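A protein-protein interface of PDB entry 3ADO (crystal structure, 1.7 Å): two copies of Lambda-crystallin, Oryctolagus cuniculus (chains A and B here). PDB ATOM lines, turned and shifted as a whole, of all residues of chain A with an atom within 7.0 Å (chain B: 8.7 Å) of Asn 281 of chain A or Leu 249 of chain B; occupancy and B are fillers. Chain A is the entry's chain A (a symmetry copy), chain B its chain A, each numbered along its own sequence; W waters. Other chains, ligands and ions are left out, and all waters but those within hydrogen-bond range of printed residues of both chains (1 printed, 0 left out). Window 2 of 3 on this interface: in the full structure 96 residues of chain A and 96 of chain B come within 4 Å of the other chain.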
ATOM      1  N   TRP A 207     -12.672  27.235   8.463  1.00  0.00           N
ATOM      2  CA  TRP A 207     -13.227  28.312   7.648  1.00  0.00           C
ATOM      3  C   TRP A 207     -13.746  29.452   8.518  1.00  0.00           C
ATOM      4  O   TRP A 207     -13.472  30.623   8.249  1.00  0.00           O
ATOM      5  CB  TRP A 207     -14.354  27.766   6.773  1.00  0.00           C
ATOM      6  CG  TRP A 207     -14.602  28.560   5.533  1.00  0.00           C
ATOM      7  CD1 TRP A 207     -15.551  29.528   5.345  1.00  0.00           C
ATOM      8  CD2 TRP A 207     -13.890  28.449   4.295  1.00  0.00           C
ATOM      9  NE1 TRP A 207     -15.474  30.023   4.063  1.00  0.00           N
ATOM     10  CE2 TRP A 207     -14.464  29.378   3.396  1.00  0.00           C
ATOM     11  CE3 TRP A 207     -12.824  27.652   3.856  1.00  0.00           C
ATOM     12  CZ2 TRP A 207     -14.005  29.533   2.084  1.00  0.00           C
ATOM     13  CZ3 TRP A 207     -12.367  27.806   2.548  1.00  0.00           C
ATOM     14  CH2 TRP A 207     -12.961  28.742   1.678  1.00  0.00           C
ATOM     15  N   PRO A 217      -5.067  32.334   7.278  1.00  0.00           N
ATOM     16  CA  PRO A 217      -5.186  31.012   6.653  1.00  0.00           C
ATOM     17  C   PRO A 217      -3.883  30.219   6.759  1.00  0.00           C
ATOM     18  O   PRO A 217      -3.897  29.015   7.013  1.00  0.00           O
ATOM     19  CB  PRO A 217      -5.538  31.347   5.206  1.00  0.00           C
ATOM     20  CG  PRO A 217      -6.328  32.619   5.345  1.00  0.00           C
ATOM     21  CD  PRO A 217      -5.512  33.396   6.356  1.00  0.00           C
ATOM     22  N   ALA A 275     -16.302  36.814   0.336  1.00  0.00           N
ATOM     23  CA  ALA A 275     -15.096  37.357   0.945  1.00  0.00           C
ATOM     24  C   ALA A 275     -14.121  36.338   1.533  1.00  0.00           C
ATOM     25  O   ALA A 275     -12.911  36.467   1.358  1.00  0.00           O
ATOM     26  CB  ALA A 275     -15.481  38.376   2.020  1.00  0.00           C
ATOM     27  N   THR A 276     -14.635  35.327   2.225  1.00  0.00           N
ATOM     28  CA  THR A 276     -13.756  34.344   2.846  1.00  0.00           C
ATOM     29  C   THR A 276     -13.051  33.424   1.857  1.00  0.00           C
ATOM     30  O   THR A 276     -11.891  33.067   2.065  1.00  0.00           O
ATOM     31  CB  THR A 276     -14.510  33.498   3.890  1.00  0.00           C
ATOM     32  OG1 THR A 276     -15.134  34.368   4.846  1.00  0.00           O
ATOM     33  CG2 THR A 276     -13.541  32.583   4.631  1.00  0.00           C
ATOM     34  N   VAL A 277     -13.730  33.039   0.782  1.00  0.00           N
ATOM     35  CA  VAL A 277     -13.083  32.174  -0.198  1.00  0.00           C
ATOM     36  C   VAL A 277     -11.982  32.975  -0.880  1.00  0.00           C
ATOM     37  O   VAL A 277     -10.929  32.439  -1.208  1.00  0.00           O
ATOM     38  CB  VAL A 277     -14.078  31.637  -1.263  1.00  0.00           C
ATOM     39  CG1 VAL A 277     -14.547  32.760  -2.172  1.00  0.00           C
ATOM     40  CG2 VAL A 277     -13.412  30.540  -2.082  1.00  0.00           C
ATOM     41  N   GLU A 278     -12.222  34.268  -1.077  1.00  0.00           N
ATOM     42  CA  GLU A 278     -11.235  35.132  -1.714  1.00  0.00           C
ATOM     43  C   GLU A 278     -10.045  35.319  -0.778  1.00  0.00           C
ATOM     44  O   GLU A 278      -8.895  35.345  -1.215  1.00  0.00           O
ATOM     45  CB  GLU A 278     -11.854  36.495  -2.052  1.00  0.00           C
ATOM     46  CG  GLU A 278     -13.142  36.402  -2.865  1.00  0.00           C
ATOM     47  CD  GLU A 278     -13.713  37.763  -3.240  1.00  0.00           C
ATOM     48  OE1 GLU A 278     -13.758  38.659  -2.369  1.00  0.00           O
ATOM     49  OE2 GLU A 278     -14.128  37.930  -4.406  1.00  0.00           O
ATOM     50  N   LYS A 279     -10.330  35.442   0.514  1.00  0.00           N
ATOM     51  CA  LYS A 279      -9.285  35.618   1.512  1.00  0.00           C
ATOM     52  C   LYS A 279      -8.453  34.347   1.622  1.00  0.00           C
ATOM     53  O   LYS A 279      -7.223  34.396   1.640  1.00  0.00           O
ATOM     54  CB  LYS A 279      -9.902  35.946   2.870  1.00  0.00           C
ATOM     55  CG  LYS A 279      -8.884  36.172   3.968  1.00  0.00           C
ATOM     56  CD  LYS A 279      -9.553  36.734   5.210  1.00  0.00           C
ATOM     57  CE  LYS A 279      -8.524  37.220   6.216  1.00  0.00           C
ATOM     58  NZ  LYS A 279      -9.166  37.999   7.311  1.00  0.00           N
ATOM     59  N   VAL A 280      -9.128  33.206   1.699  1.00  0.00           N
ATOM     60  CA  VAL A 280      -8.421  31.936   1.797  1.00  0.00           C
ATOM     61  C   VAL A 280      -7.657  31.654   0.506  1.00  0.00           C
ATOM     62  O   VAL A 280      -6.494  31.264   0.541  1.00  0.00           O
ATOM     63  CB  VAL A 280      -9.390  30.766   2.078  1.00  0.00           C
ATOM     64  CG1 VAL A 280      -8.635  29.442   2.019  1.00  0.00           C
ATOM     65  CG2 VAL A 280     -10.030  30.939   3.451  1.00  0.00           C
ATOM     66  N   ASN A 281      -8.307  31.863  -0.637  1.00  0.00           N
ATOM     67  CA  ASN A 281      -7.653  31.615  -1.918  1.00  0.00           C
ATOM     68  C   ASN A 281      -6.409  32.481  -2.096  1.00  0.00           C
ATOM     69  O   ASN A 281      -5.369  31.995  -2.535  1.00  0.00           O
ATOM     70  CB  ASN A 281      -8.612  31.868  -3.082  1.00  0.00           C
ATOM     71  CG  ASN A 281      -7.983  31.552  -4.429  1.00  0.00           C
ATOM     72  OD1 ASN A 281      -7.594  30.413  -4.694  1.00  0.00           O
ATOM     73  ND2 ASN A 281      -7.871  32.564  -5.284  1.00  0.00           N
ATOM     74  N   GLN A 282      -6.511  33.763  -1.755  1.00  0.00           N
ATOM     75  CA  GLN A 282      -5.371  34.662  -1.892  1.00  0.00           C
ATOM     76  C   GLN A 282      -4.186  34.190  -1.059  1.00  0.00           C
ATOM     77  O   GLN A 282      -3.041  34.272  -1.498  1.00  0.00           O
ATOM     78  CB  GLN A 282      -5.758  36.090  -1.491  1.00  0.00           C
ATOM     79  CG  GLN A 282      -6.678  36.767  -2.496  1.00  0.00           C
ATOM     80  CD  GLN A 282      -7.070  38.176  -2.092  1.00  0.00           C
ATOM     81  OE1 GLN A 282      -7.744  38.881  -2.845  1.00  0.00           O
ATOM     82  NE2 GLN A 282      -6.654  38.594  -0.898  1.00  0.00           N
ATOM     83  N   ALA A 283      -4.463  33.685   0.138  1.00  0.00           N
ATOM     84  CA  ALA A 283      -3.401  33.196   1.009  1.00  0.00           C
ATOM     85  C   ALA A 283      -2.794  31.912   0.446  1.00  0.00           C
ATOM     86  O   ALA A 283      -1.577  31.727   0.479  1.00  0.00           O
ATOM     87  CB  ALA A 283      -3.941  32.955   2.413  1.00  0.00           C
ATOM     88  N   MET A 284      -3.644  31.030  -0.074  1.00  0.00           N
ATOM     89  CA  MET A 284      -3.168  29.776  -0.643  1.00  0.00           C
ATOM     90  C   MET A 284      -2.316  30.038  -1.881  1.00  0.00           C
ATOM     91  O   MET A 284      -1.283  29.398  -2.077  1.00  0.00           O
ATOM     92  CB  MET A 284      -4.346  28.861  -1.010  1.00  0.00           C
ATOM     93  CG  MET A 284      -5.167  28.362   0.179  1.00  0.00           C
ATOM     94  SD  MET A 284      -4.201  27.453   1.416  1.00  0.00           S
ATOM     95  CE  MET A 284      -4.034  28.700   2.694  1.00  0.00           C
ATOM     96  N   CYS A 285      -2.741  30.986  -2.711  1.00  0.00           N
ATOM     97  CA  CYS A 285      -1.995  31.303  -3.923  1.00  0.00           C
ATOM     98  C   CYS A 285      -0.656  31.975  -3.645  1.00  0.00           C
ATOM     99  O   CYS A 285       0.272  31.864  -4.448  1.00  0.00           O
ATOM    100  CB  CYS A 285      -2.838  32.172  -4.856  1.00  0.00           C
ATOM    101  SG  CYS A 285      -4.209  31.277  -5.625  1.00  0.00           S
ATOM    102  N   LYS A 286      -0.551  32.669  -2.516  1.00  0.00           N
ATOM    103  CA  LYS A 286       0.699  33.324  -2.154  1.00  0.00           C
ATOM    104  C   LYS A 286       1.746  32.249  -1.878  1.00  0.00           C
ATOM    105  O   LYS A 286       2.919  32.402  -2.218  1.00  0.00           O
ATOM    106  CB  LYS A 286       0.513  34.196  -0.910  1.00  0.00           C
ATOM    107  CG  LYS A 286       1.788  34.893  -0.453  1.00  0.00           C
ATOM    108  CD  LYS A 286       1.536  35.815   0.732  1.00  0.00           C
ATOM    109  CE  LYS A 286       0.607  36.962   0.360  1.00  0.00           C
ATOM    110  NZ  LYS A 286       1.186  37.830  -0.707  1.00  0.00           N
ATOM    111  N   LYS A 287       1.300  31.157  -1.263  1.00  0.00           N
ATOM    112  CA  LYS A 287       2.163  30.031  -0.927  1.00  0.00           C
ATOM    113  C   LYS A 287       2.395  29.149  -2.149  1.00  0.00           C
ATOM    114  O   LYS A 287       3.514  28.703  -2.407  1.00  0.00           O
ATOM    115  CB  LYS A 287       1.517  29.188   0.178  1.00  0.00           C
ATOM    116  CG  LYS A 287       1.325  29.915   1.497  1.00  0.00           C
ATOM    117  CD  LYS A 287       0.272  29.229   2.367  1.00  0.00           C
ATOM    118  CE  LYS A 287       0.625  27.780   2.677  1.00  0.00           C
ATOM    119  NZ  LYS A 287      -0.449  27.105   3.478  1.00  0.00           N
ATOM    120  N   VAL A 288       1.324  28.900  -2.895  1.00  0.00           N
ATOM    121  CA  VAL A 288       1.388  28.063  -4.086  1.00  0.00           C
ATOM    122  C   VAL A 288       0.538  28.637  -5.220  1.00  0.00           C
ATOM    123  O   VAL A 288      -0.682  28.470  -5.230  1.00  0.00           O
ATOM    124  CB  VAL A 288       0.879  26.634  -3.780  1.00  0.00           C
ATOM    125  CG1 VAL A 288       1.002  25.756  -5.017  1.00  0.00           C
ATOM    126  CG2 VAL A 288       1.665  26.039  -2.623  1.00  0.00           C
ATOM    127  N   ALA A 290      -1.736  29.234  -8.206  1.00  0.00           N
ATOM    128  CA  ALA A 290      -2.729  28.312  -8.743  1.00  0.00           C
ATOM    129  C   ALA A 290      -2.590  27.961 -10.220  1.00  0.00           C
ATOM    130  O   ALA A 290      -3.587  27.889 -10.939  1.00  0.00           O
ATOM    131  CB  ALA A 290      -4.128  28.853  -8.470  1.00  0.00           C
ATOM    132  N   LEU B 238      -6.494  23.695   4.653  1.00  0.00           N
ATOM    133  CA  LEU B 238      -6.794  24.626   3.570  1.00  0.00           C
ATOM    134  C   LEU B 238      -5.892  24.374   2.368  1.00  0.00           C
ATOM    135  O   LEU B 238      -6.371  24.278   1.237  1.00  0.00           O
ATOM    136  CB  LEU B 238      -6.653  26.072   4.057  1.00  0.00           C
ATOM    137  CG  LEU B 238      -7.545  26.412   5.254  1.00  0.00           C
ATOM    138  CD1 LEU B 238      -7.343  27.869   5.662  1.00  0.00           C
ATOM    139  CD2 LEU B 238      -9.008  26.141   4.896  1.00  0.00           C
ATOM    140  N   MET B 241      -6.951  21.385   0.494  1.00  0.00           N
ATOM    141  CA  MET B 241      -8.041  21.602  -0.456  1.00  0.00           C
ATOM    142  C   MET B 241      -7.464  22.185  -1.749  1.00  0.00           C
ATOM    143  O   MET B 241      -7.824  21.779  -2.854  1.00  0.00           O
ATOM    144  CB  MET B 241      -9.055  22.596   0.122  1.00  0.00           C
ATOM    145  CG  MET B 241      -9.762  22.134   1.378  1.00  0.00           C
ATOM    146  SD  MET B 241     -10.573  23.512   2.227  1.00  0.00           S
ATOM    147  CE  MET B 241     -12.001  23.753   1.209  1.00  0.00           C
ATOM    148  N   HIS B 242      -6.567  23.151  -1.579  1.00  0.00           N
ATOM    149  CA  HIS B 242      -5.904  23.853  -2.677  1.00  0.00           C
ATOM    150  C   HIS B 242      -5.225  22.896  -3.657  1.00  0.00           C
ATOM    151  O   HIS B 242      -5.296  23.074  -4.882  1.00  0.00           O
ATOM    152  CB  HIS B 242      -4.863  24.807  -2.083  1.00  0.00           C
ATOM    153  CG  HIS B 242      -4.316  25.811  -3.050  1.00  0.00           C
ATOM    154  ND1 HIS B 242      -5.097  26.780  -3.642  1.00  0.00           N
ATOM    155  CD2 HIS B 242      -3.047  26.046  -3.463  1.00  0.00           C
ATOM    156  CE1 HIS B 242      -4.333  27.573  -4.374  1.00  0.00           C
ATOM    157  NE2 HIS B 242      -3.085  27.150  -4.281  1.00  0.00           N
ATOM    158  N   LEU B 243      -4.569  21.878  -3.110  1.00  0.00           N
ATOM    159  CA  LEU B 243      -3.850  20.903  -3.922  1.00  0.00           C
ATOM    160  C   LEU B 243      -4.704  19.739  -4.416  1.00  0.00           C
ATOM    161  O   LEU B 243      -4.319  19.056  -5.363  1.00  0.00           O
ATOM    162  CB  LEU B 243      -2.657  20.344  -3.138  1.00  0.00           C
ATOM    163  CG  LEU B 243      -1.640  21.335  -2.570  1.00  0.00           C
ATOM    164  CD1 LEU B 243      -0.557  20.572  -1.807  1.00  0.00           C
ATOM    165  CD2 LEU B 243      -1.021  22.151  -3.698  1.00  0.00           C
ATOM    166  N   ALA B 245      -7.457  19.932  -5.894  1.00  0.00           N
ATOM    167  CA  ALA B 245      -8.259  20.444  -7.000  1.00  0.00           C
ATOM    168  C   ALA B 245      -7.308  21.401  -7.700  1.00  0.00           C
ATOM    169  O   ALA B 245      -6.125  21.446  -7.367  1.00  0.00           O
ATOM    170  CB  ALA B 245      -9.489  21.185  -6.487  1.00  0.00           C
ATOM    171  N   GLU B 246      -7.796  22.155  -8.675  1.00  0.00           N
ATOM    172  CA  GLU B 246      -6.915  23.089  -9.354  1.00  0.00           C
ATOM    173  C   GLU B 246      -6.933  24.416  -8.609  1.00  0.00           C
ATOM    174  O   GLU B 246      -7.196  25.466  -9.193  1.00  0.00           O
ATOM    175  CB  GLU B 246      -7.357  23.282 -10.806  1.00  0.00           C
ATOM    176  CG  GLU B 246      -7.283  22.007 -11.635  1.00  0.00           C
ATOM    177  CD  GLU B 246      -5.933  21.318 -11.525  1.00  0.00           C
ATOM    178  OE1 GLU B 246      -4.911  21.935 -11.895  1.00  0.00           O
ATOM    179  OE2 GLU B 246      -5.894  20.158 -11.064  1.00  0.00           O
ATOM    180  N   GLY B 247      -6.646  24.356  -7.311  1.00  0.00           N
ATOM    181  CA  GLY B 247      -6.636  25.558  -6.499  1.00  0.00           C
ATOM    182  C   GLY B 247      -7.859  25.624  -5.606  1.00  0.00           C
ATOM    183  O   GLY B 247      -8.811  24.872  -5.798  1.00  0.00           O
ATOM    184  N   MET B 248      -7.840  26.533  -4.635  1.00  0.00           N
ATOM    185  CA  MET B 248      -8.953  26.684  -3.698  1.00  0.00           C
ATOM    186  C   MET B 248     -10.298  26.991  -4.363  1.00  0.00           C
ATOM    187  O   MET B 248     -11.327  26.416  -3.995  1.00  0.00           O
ATOM    188  CB  MET B 248      -8.623  27.778  -2.680  1.00  0.00           C
ATOM    189  CG  MET B 248      -9.719  28.057  -1.659  1.00  0.00           C
ATOM    190  SD  MET B 248     -10.141  26.644  -0.595  1.00  0.00           S
ATOM    191  CE  MET B 248      -8.544  26.277   0.102  1.00  0.00           C
ATOM    192  N   LEU B 249     -10.299  27.908  -5.326  1.00  0.00           N
ATOM    193  CA  LEU B 249     -11.537  28.260  -6.012  1.00  0.00           C
ATOM    194  C   LEU B 249     -12.102  27.012  -6.678  1.00  0.00           C
ATOM    195  O   LEU B 249     -13.304  26.754  -6.618  1.00  0.00           O
ATOM    196  CB  LEU B 249     -11.280  29.343  -7.066  1.00  0.00           C
ATOM    197  CG  LEU B 249     -10.664  30.659  -6.576  1.00  0.00           C
ATOM    198  CD1 LEU B 249     -10.465  31.601  -7.762  1.00  0.00           C
ATOM    199  CD2 LEU B 249     -11.566  31.302  -5.516  1.00  0.00           C
ATOM    200  N   SER B 250     -11.220  26.240  -7.305  1.00  0.00           N
ATOM    201  CA  SER B 250     -11.604  25.007  -7.981  1.00  0.00           C
ATOM    202  C   SER B 250     -12.190  24.000  -6.993  1.00  0.00           C
ATOM    203  O   SER B 250     -13.209  23.367  -7.267  1.00  0.00           O
ATOM    204  CB  SER B 250     -10.385  24.399  -8.681  1.00  0.00           C
ATOM    205  OG  SER B 250     -10.699  23.150  -9.273  1.00  0.00           O
ATOM    206  N   TYR B 251     -11.550  23.853  -5.838  1.00  0.00           N
ATOM    207  CA  TYR B 251     -12.042  22.898  -4.828  1.00  0.00           C
ATOM    208  C   TYR B 251     -13.439  23.266  -4.361  1.00  0.00           C
ATOM    209  O   TYR B 251     -14.313  22.426  -4.234  1.00  0.00           O
ATOM    210  CB  TYR B 251     -11.081  22.865  -3.620  1.00  0.00           C
ATOM    211  CG  TYR B 251     -11.418  21.716  -2.703  1.00  0.00           C
ATOM    212  CD1 TYR B 251     -10.772  20.484  -2.859  1.00  0.00           C
ATOM    213  CD2 TYR B 251     -12.367  21.857  -1.684  1.00  0.00           C
ATOM    214  CE1 TYR B 251     -11.090  19.412  -2.029  1.00  0.00           C
ATOM    215  CE2 TYR B 251     -12.682  20.780  -0.858  1.00  0.00           C
ATOM    216  CZ  TYR B 251     -12.047  19.564  -1.031  1.00  0.00           C
ATOM    217  OH  TYR B 251     -12.356  18.489  -0.214  1.00  0.00           O
ATOM    218  N   CYS B 252     -13.621  24.568  -4.063  1.00  0.00           N
ATOM    219  CA  CYS B 252     -14.927  25.022  -3.602  1.00  0.00           C
ATOM    220  C   CYS B 252     -15.973  24.885  -4.702  1.00  0.00           C
ATOM    221  O   CYS B 252     -17.134  24.585  -4.459  1.00  0.00           O
ATOM    222  CB  CYS B 252     -14.796  26.489  -3.188  1.00  0.00           C
ATOM    223  SG  CYS B 252     -13.906  26.680  -1.626  1.00  0.00           S
ATOM    224  N   ASP B 253     -15.569  25.073  -5.959  1.00  0.00           N
ATOM    225  CA  ASP B 253     -16.506  24.933  -7.080  1.00  0.00           C
ATOM    226  C   ASP B 253     -16.957  23.482  -7.227  1.00  0.00           C
ATOM    227  O   ASP B 253     -18.132  23.198  -7.465  1.00  0.00           O
ATOM    228  CB  ASP B 253     -15.865  25.350  -8.410  1.00  0.00           C
ATOM    229  CG  ASP B 253     -15.701  26.846  -8.544  1.00  0.00           C
ATOM    230  OD1 ASP B 253     -16.467  27.597  -7.904  1.00  0.00           O
ATOM    231  OD2 ASP B 253     -14.813  27.268  -9.315  1.00  0.00           O
ATOM    232  N   ARG B 254     -16.009  22.564  -7.093  1.00  0.00           N
ATOM    233  CA  ARG B 254     -16.297  21.146  -7.238  1.00  0.00           C
ATOM    234  C   ARG B 254     -16.979  20.477  -6.048  1.00  0.00           C
ATOM    235  O   ARG B 254     -17.872  19.648  -6.229  1.00  0.00           O
ATOM    236  CB  ARG B 254     -15.004  20.381  -7.541  1.00  0.00           C
ATOM    237  CG  ARG B 254     -14.325  20.768  -8.844  1.00  0.00           C
ATOM    238  CD  ARG B 254     -13.026  19.999  -9.040  1.00  0.00           C
ATOM    239  NE  ARG B 254     -12.354  20.371 -10.283  1.00  0.00           N
ATOM    240  CZ  ARG B 254     -11.139  19.957 -10.630  1.00  0.00           C
ATOM    241  NH1 ARG B 254     -10.454  19.150  -9.825  1.00  0.00           N
ATOM    242  NH2 ARG B 254     -10.609  20.347 -11.782  1.00  0.00           N
ATOM    243  N   TYR B 255     -16.576  20.848  -4.837  1.00  0.00           N
ATOM    244  CA  TYR B 255     -17.094  20.192  -3.642  1.00  0.00           C
ATOM    245  C   TYR B 255     -17.878  20.981  -2.592  1.00  0.00           C
ATOM    246  O   TYR B 255     -18.330  20.394  -1.610  1.00  0.00           O
ATOM    247  CB  TYR B 255     -15.925  19.488  -2.950  1.00  0.00           C
ATOM    248  CG  TYR B 255     -15.075  18.668  -3.893  1.00  0.00           C
ATOM    249  CD1 TYR B 255     -15.581  17.519  -4.497  1.00  0.00           C
ATOM    250  CD2 TYR B 255     -13.765  19.048  -4.193  1.00  0.00           C
ATOM    251  CE1 TYR B 255     -14.805  16.766  -5.378  1.00  0.00           C
ATOM    252  CE2 TYR B 255     -12.980  18.303  -5.072  1.00  0.00           C
ATOM    253  CZ  TYR B 255     -13.508  17.161  -5.661  1.00  0.00           C
ATOM    254  OH  TYR B 255     -12.738  16.420  -6.535  1.00  0.00           O
ATOM    255  N   SER B 256     -18.053  22.288  -2.771  1.00  0.00           N
ATOM    256  CA  SER B 256     -18.784  23.056  -1.765  1.00  0.00           C
ATOM    257  C   SER B 256     -20.204  22.531  -1.561  1.00  0.00           C
ATOM    258  O   SER B 256     -20.706  22.517  -0.440  1.00  0.00           O
ATOM    259  CB  SER B 256     -18.830  24.544  -2.133  1.00  0.00           C
ATOM    260  OG  SER B 256     -19.622  24.768  -3.281  1.00  0.00           O
HETATM  261  O   HOH W   1      -6.244  26.753 -11.522  1.00  0.00           O
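O of His 242 of chain B lies within hydrogen-bond range of N of Gly 247 of chain B (3.1 Å).
The backbone NH (N) of Met 248 of chain B is in hydrogen-bond range of a ring nitrogen (ND1) of His 242 of chain B, at 2.9 Å.
The backbone carbonyl oxygen of Met 248 of chain B is in hydrogen-bond range of the side-chain sulfur of Cys 252 of chain B, 3.5 Å away.
The backbone carbonyl oxygen (O) of Cys 252 of chain B sits at hydrogen-bond distance from the side-chain hydroxyl (OG) of Ser 256 of chain B (2.8 Å).
The backbone carbonyl oxygen of Asn 281 of chain A is in hydrogen-bond range of the side-chain sulfur of Cys 285 of chain A.
Hydrophobic or aromatic side chains of chain A that line the printed part of chain B: Pro 217, Val 277, Val 280, Met 284 and Val 288.
Hydrophobic or aromatic side chains of chain B that line the printed part of chain A: Leu 238, His 242, Met 248 and Leu 249.
Among the printed residues, 11 pairs touch across the chains.
Water W1 bridges the backbone carbonyl oxygen (O) of Glu 246 of chain B and the backbone carbonyl oxygen (O) of Ala 290 of chain A.
No position is printed for both chains.
Of the 11 pairs that touch across the chains among the printed residues, none has its exchanged pair printed and touching as well.
Among the printed residues, merely in contact across the chains: Pro 217 of chain A with Leu 238 of chain B (3.9 Å), Val 277 of chain A with Leu 249 of chain B (3.97 Å), Val 277 of chain A with Cys 252 of chain B (3.9 Å), Val 280 of chain A with Met 248 of chain B (3.7 Å), Asn 281 of chain A with Met 248 of chain B (3.5 Å), Asn 281 of chain A with Leu 249 of chain B (3.5 Å), Met 284 of chain A with Leu 238 of chain B (3.6 Å), Met 284 of chain A with His 242 of chain B (3.4 Å), Met 284 of chain A with Met 248 of chain B (3.97 Å) and Cys 285 of chain A with His 242 of chain B (3.9 Å).
Of the printed residues of chain B, Val 277 of chain A touches Leu 249 and Cys 252.
Of chain B, only Met 248 comes within 4 Å of Val 280 of chain A.
Of the printed residues of chain B, Asn 281 of chain A touches Met 248 and Leu 249.
Gln 282 of chain A touches none of the printed residues of chain B.
Printed residues of chain B within 4 Å of Cys 285 of chain A: His 242.
Of the printed residues of chain B, Val 288 of chain A touches His 242 (2.9 Å).
Printed residues of chain A within 4 Å of Met 248 of chain B: Val 280 (3.7 Å), Asn 281 (3.5 Å) and Met 284 (3.97 Å).
Leu 249 of chain B touches just these residues of chain A: Val 277 (3.97 Å) and Asn 281 (3.5 Å).
Tyr 251 of chain B touches none of the printed residues of chain A.
The nearest residue of chain B that does not touch Asn 281 of chain A is His 242 of chain B (4.3 Å).
The backbone carbonyl oxygen of Val 288 of chain A sits at hydrogen-bond distance from a ring nitrogen (NE2) of His 242 of chain B (2.9 Å).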
